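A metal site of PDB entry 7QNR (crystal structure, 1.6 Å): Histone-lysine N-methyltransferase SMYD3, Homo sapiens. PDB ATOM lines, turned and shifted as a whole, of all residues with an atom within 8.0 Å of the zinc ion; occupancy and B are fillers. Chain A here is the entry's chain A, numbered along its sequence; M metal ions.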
ATOM      1  N   VAL A  51      -4.113  27.467 -11.374  1.00  0.00           N
ATOM      2  CA  VAL A  51      -3.976  27.194 -12.793  1.00  0.00           C
ATOM      3  C   VAL A  51      -4.991  26.127 -13.182  1.00  0.00           C
ATOM      4  O   VAL A  51      -5.450  25.338 -12.353  1.00  0.00           O
ATOM      5  CB  VAL A  51      -2.538  26.759 -13.171  1.00  0.00           C
ATOM      6  CG1 VAL A  51      -1.514  27.770 -12.689  1.00  0.00           C
ATOM      7  CG2 VAL A  51      -2.228  25.370 -12.632  1.00  0.00           C
ATOM      8  N   CYS A  52      -5.321  26.112 -14.471  1.00  0.00           N
ATOM      9  CA  CYS A  52      -6.235  25.113 -15.010  1.00  0.00           C
ATOM     10  C   CYS A  52      -5.617  23.717 -14.903  1.00  0.00           C
ATOM     11  O   CYS A  52      -4.460  23.508 -15.265  1.00  0.00           O
ATOM     12  CB  CYS A  52      -6.542  25.451 -16.468  1.00  0.00           C
ATOM     13  SG  CYS A  52      -7.497  24.244 -17.342  1.00  0.00           S
ATOM     14  N   ASP A  53      -6.410  22.751 -14.435  1.00  0.00           N
ATOM     15  CA  ASP A  53      -5.898  21.402 -14.264  1.00  0.00           C
ATOM     16  C   ASP A  53      -5.392  20.814 -15.568  1.00  0.00           C
ATOM     17  O   ASP A  53      -4.496  19.958 -15.560  1.00  0.00           O
ATOM     18  CB  ASP A  53      -6.963  20.469 -13.693  1.00  0.00           C
ATOM     19  CG  ASP A  53      -7.002  20.450 -12.176  1.00  0.00           C
ATOM     20  OD1 ASP A  53      -6.703  21.475 -11.540  1.00  0.00           O
ATOM     21  OD2 ASP A  53      -7.287  19.361 -11.616  1.00  0.00           O
ATOM     22  N   ARG A  54      -5.956  21.232 -16.700  1.00  0.00           N
ATOM     23  CA  ARG A  54      -5.581  20.635 -17.988  1.00  0.00           C
ATOM     24  C   ARG A  54      -4.412  21.374 -18.633  1.00  0.00           C
ATOM     25  O   ARG A  54      -3.357  20.786 -18.849  1.00  0.00           O
ATOM     26  CB  ARG A  54      -6.785  20.640 -18.926  1.00  0.00           C
ATOM     27  CG  ARG A  54      -6.600  19.771 -20.161  1.00  0.00           C
ATOM     28  CD  ARG A  54      -6.287  20.638 -21.362  1.00  0.00           C
ATOM     29  NE  ARG A  54      -6.336  19.903 -22.619  1.00  0.00           N
ATOM     30  CZ  ARG A  54      -6.462  20.468 -23.812  1.00  0.00           C
ATOM     31  NH1 ARG A  54      -6.476  19.745 -24.925  1.00  0.00           N
ATOM     32  NH2 ARG A  54      -6.587  21.793 -23.905  1.00  0.00           N
ATOM     33  N   CYS A  55      -4.581  22.654 -18.943  1.00  0.00           N
ATOM     34  CA  CYS A  55      -3.573  23.389 -19.703  1.00  0.00           C
ATOM     35  C   CYS A  55      -2.524  24.069 -18.814  1.00  0.00           C
ATOM     36  O   CYS A  55      -1.518  24.556 -19.344  1.00  0.00           O
ATOM     37  CB  CYS A  55      -4.257  24.437 -20.595  1.00  0.00           C
ATOM     38  SG  CYS A  55      -5.044  25.805 -19.725  1.00  0.00           S
ATOM     39  N   LEU A  56      -2.733  24.102 -17.502  1.00  0.00           N
ATOM     40  CA  LEU A  56      -1.742  24.610 -16.552  1.00  0.00           C
ATOM     41  C   LEU A  56      -1.462  26.089 -16.757  1.00  0.00           C
ATOM     42  O   LEU A  56      -0.355  26.552 -16.475  1.00  0.00           O
ATOM     43  CB  LEU A  56      -0.441  23.809 -16.632  1.00  0.00           C
ATOM     44  CG  LEU A  56      -0.553  22.287 -16.441  1.00  0.00           C
ATOM     45  CD1 LEU A  56       0.802  21.606 -16.625  1.00  0.00           C
ATOM     46  CD2 LEU A  56      -1.121  21.976 -15.077  1.00  0.00           C
ATOM     47  N   LEU A  57      -2.446  26.838 -17.237  1.00  0.00           N
ATOM     48  CA  LEU A  57      -2.358  28.292 -17.334  1.00  0.00           C
ATOM     49  C   LEU A  57      -3.085  28.934 -16.154  1.00  0.00           C
ATOM     50  O   LEU A  57      -4.108  28.428 -15.690  1.00  0.00           O
ATOM     51  CB  LEU A  57      -2.949  28.793 -18.644  1.00  0.00           C
ATOM     52  CG  LEU A  57      -2.267  28.350 -19.938  1.00  0.00           C
ATOM     53  CD1 LEU A  57      -2.970  28.981 -21.143  1.00  0.00           C
ATOM     54  CD2 LEU A  57      -0.803  28.710 -19.943  1.00  0.00           C
ATOM     55  N   GLY A  58      -2.542  30.059 -15.688  1.00  0.00           N
ATOM     56  CA  GLY A  58      -3.137  30.766 -14.573  1.00  0.00           C
ATOM     57  C   GLY A  58      -4.153  31.812 -15.001  1.00  0.00           C
ATOM     58  O   GLY A  58      -3.851  32.994 -15.040  1.00  0.00           O
ATOM     59  N   LYS A  59      -5.377  31.366 -15.305  1.00  0.00           N
ATOM     60  CA  LYS A  59      -6.440  32.296 -15.643  1.00  0.00           C
ATOM     61  C   LYS A  59      -6.918  33.036 -14.394  1.00  0.00           C
ATOM     62  O   LYS A  59      -6.727  32.590 -13.263  1.00  0.00           O
ATOM     63  CB  LYS A  59      -7.634  31.566 -16.266  1.00  0.00           C
ATOM     64  CG  LYS A  59      -7.387  30.812 -17.571  1.00  0.00           C
ATOM     65  CD  LYS A  59      -6.500  31.530 -18.574  1.00  0.00           C
ATOM     66  CE  LYS A  59      -6.504  30.758 -19.894  1.00  0.00           C
ATOM     67  NZ  LYS A  59      -6.139  31.589 -21.081  1.00  0.00           N
ATOM     68  N   LEU A  62     -11.463  30.535 -12.886  1.00  0.00           N
ATOM     69  CA  LEU A  62     -11.412  29.091 -13.024  1.00  0.00           C
ATOM     70  C   LEU A  62     -12.688  28.509 -12.434  1.00  0.00           C
ATOM     71  O   LEU A  62     -13.172  28.977 -11.398  1.00  0.00           O
ATOM     72  CB  LEU A  62     -10.195  28.495 -12.303  1.00  0.00           C
ATOM     73  CG  LEU A  62      -8.810  28.858 -12.855  1.00  0.00           C
ATOM     74  CD1 LEU A  62      -7.719  28.217 -12.000  1.00  0.00           C
ATOM     75  CD2 LEU A  62      -8.670  28.438 -14.309  1.00  0.00           C
ATOM     76  N   LYS A  72      -9.900  22.318 -11.128  1.00  0.00           N
ATOM     77  CA  LYS A  72     -10.398  23.577 -11.646  1.00  0.00           C
ATOM     78  C   LYS A  72      -9.963  23.733 -13.095  1.00  0.00           C
ATOM     79  O   LYS A  72      -8.876  23.282 -13.473  1.00  0.00           O
ATOM     80  CB  LYS A  72      -9.909  24.772 -10.823  1.00  0.00           C
ATOM     81  CG  LYS A  72     -10.242  24.667  -9.346  1.00  0.00           C
ATOM     82  CD  LYS A  72     -10.484  26.040  -8.738  1.00  0.00           C
ATOM     83  CE  LYS A  72     -10.608  25.963  -7.217  1.00  0.00           C
ATOM     84  NZ  LYS A  72     -10.745  27.315  -6.593  1.00  0.00           N
ATOM     85  N   TYR A  73     -10.818  24.351 -13.901  1.00  0.00           N
ATOM     86  CA  TYR A  73     -10.612  24.424 -15.341  1.00  0.00           C
ATOM     87  C   TYR A  73     -10.857  25.840 -15.829  1.00  0.00           C
ATOM     88  O   TYR A  73     -11.679  26.586 -15.285  1.00  0.00           O
ATOM     89  CB  TYR A  73     -11.551  23.455 -16.080  1.00  0.00           C
ATOM     90  CG  TYR A  73     -11.299  22.011 -15.727  1.00  0.00           C
ATOM     91  CD1 TYR A  73     -10.143  21.368 -16.148  1.00  0.00           C
ATOM     92  CD2 TYR A  73     -12.216  21.297 -14.979  1.00  0.00           C
ATOM     93  CE1 TYR A  73      -9.901  20.033 -15.821  1.00  0.00           C
ATOM     94  CE2 TYR A  73     -11.984  19.972 -14.654  1.00  0.00           C
ATOM     95  CZ  TYR A  73     -10.833  19.356 -15.063  1.00  0.00           C
ATOM     96  OH  TYR A  73     -10.604  18.027 -14.747  1.00  0.00           O
ATOM     97  N   CYS A  74     -10.117  26.211 -16.881  1.00  0.00           N
ATOM     98  CA  CYS A  74     -10.283  27.521 -17.490  1.00  0.00           C
ATOM     99  C   CYS A  74     -11.448  27.591 -18.457  1.00  0.00           C
ATOM    100  O   CYS A  74     -11.883  28.711 -18.803  1.00  0.00           O
ATOM    101  CB  CYS A  74      -8.992  27.899 -18.217  1.00  0.00           C
ATOM    102  SG  CYS A  74      -8.761  27.009 -19.772  1.00  0.00           S
ATOM    103  N   SER A  75     -11.984  26.460 -18.889  1.00  0.00           N
ATOM    104  CA  SER A  75     -12.970  26.471 -19.957  1.00  0.00           C
ATOM    105  C   SER A  75     -13.660  25.113 -20.026  1.00  0.00           C
ATOM    106  O   SER A  75     -13.159  24.118 -19.484  1.00  0.00           O
ATOM    107  CB  SER A  75     -12.307  26.770 -21.306  1.00  0.00           C
ATOM    108  OG  SER A  75     -11.314  25.786 -21.593  1.00  0.00           O
ATOM    109  N   ALA A  76     -14.796  25.088 -20.719  1.00  0.00           N
ATOM    110  CA  ALA A  76     -15.445  23.819 -21.034  1.00  0.00           C
ATOM    111  C   ALA A  76     -14.529  22.939 -21.882  1.00  0.00           C
ATOM    112  O   ALA A  76     -14.520  21.710 -21.734  1.00  0.00           O
ATOM    113  CB  ALA A  76     -16.768  24.068 -21.759  1.00  0.00           C
ATOM    114  N   LYS A  77     -13.761  23.551 -22.792  1.00  0.00           N
ATOM    115  CA  LYS A  77     -12.842  22.774 -23.609  1.00  0.00           C
ATOM    116  C   LYS A  77     -11.859  22.001 -22.743  1.00  0.00           C
ATOM    117  O   LYS A  77     -11.634  20.808 -22.954  1.00  0.00           O
ATOM    118  CB  LYS A  77     -12.085  23.706 -24.563  1.00  0.00           C
ATOM    119  CG  LYS A  77     -11.103  22.985 -25.479  1.00  0.00           C
ATOM    120  CD  LYS A  77     -10.296  23.979 -26.327  1.00  0.00           C
ATOM    121  CE  LYS A  77      -9.419  23.245 -27.335  1.00  0.00           C
ATOM    122  NZ  LYS A  77      -8.506  24.165 -28.064  1.00  0.00           N
ATOM    123  N   CYS A  78     -11.241  22.682 -21.761  1.00  0.00           N
ATOM    124  CA  CYS A  78     -10.257  22.009 -20.919  1.00  0.00           C
ATOM    125  C   CYS A  78     -10.911  20.967 -20.022  1.00  0.00           C
ATOM    126  O   CYS A  78     -10.319  19.911 -19.771  1.00  0.00           O
ATOM    127  CB  CYS A  78      -9.479  23.013 -20.086  1.00  0.00           C
ATOM    128  SG  CYS A  78      -8.111  23.750 -20.976  1.00  0.00           S
ATOM    129  N   GLN A  79     -12.118  21.240 -19.541  1.00  0.00           N
ATOM    130  CA  GLN A  79     -12.806  20.243 -18.712  1.00  0.00           C
ATOM    131  C   GLN A  79     -13.065  18.964 -19.501  1.00  0.00           C
ATOM    132  O   GLN A  79     -12.961  17.856 -18.947  1.00  0.00           O
ATOM    133  CB  GLN A  79     -14.126  20.827 -18.185  1.00  0.00           C
ATOM    134  CG  GLN A  79     -14.921  19.912 -17.263  1.00  0.00           C
ATOM    135  CD  GLN A  79     -15.715  18.843 -18.018  1.00  0.00           C
ATOM    136  OE1 GLN A  79     -16.103  19.030 -19.169  1.00  0.00           O
ATOM    137  NE2 GLN A  79     -15.953  17.721 -17.342  1.00  0.00           N
HETATM  138 ZN    ZN M   1      -7.282  25.196 -19.487  1.00  0.00          ZN
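Within 4 Å of the zinc ion: Cys 52, Cys 55, Cys 74 and Cys 78.
Along chain A the residues within 4 Å of the zinc ion span positions 52 to 78.
The nearest printed residue that does not touch the zinc ion is Ser 75 (4.6 Å).
The backbone NH of Cys 78 lies within hydrogen-bond range of the side-chain hydroxyl of Ser 75.
The side-chain sulfur of Cys 55 lies close to the backbone NH of Leu 57 (3.7 Å).
The side-chain sulfur (SG) of Cys 52 lies close to the backbone NH (N) of Arg 54, 3.4 Å away.
The backbone NH (N) of Cys 52 lies within hydrogen-bond range of the backbone carbonyl oxygen (O) of Leu 57 (2.9 Å).
The side-chain sulfur (SG) of Cys 74 sits close to the side-chain hydroxyl (OG) of Ser 75, 3.4 Å away.
The zinc ion is bound by the side-chain sulfur (SG) of Cys 78 (2.2 Å).
SG of Cys 55 is bound to the zinc ion (2.3 Å).
The zinc ion is bound by SG of Cys 52.
The side-chain sulfur (SG) of Cys 74 binds the zinc ion (2.4 Å).
The zinc ion has four donor atoms within binding distance.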
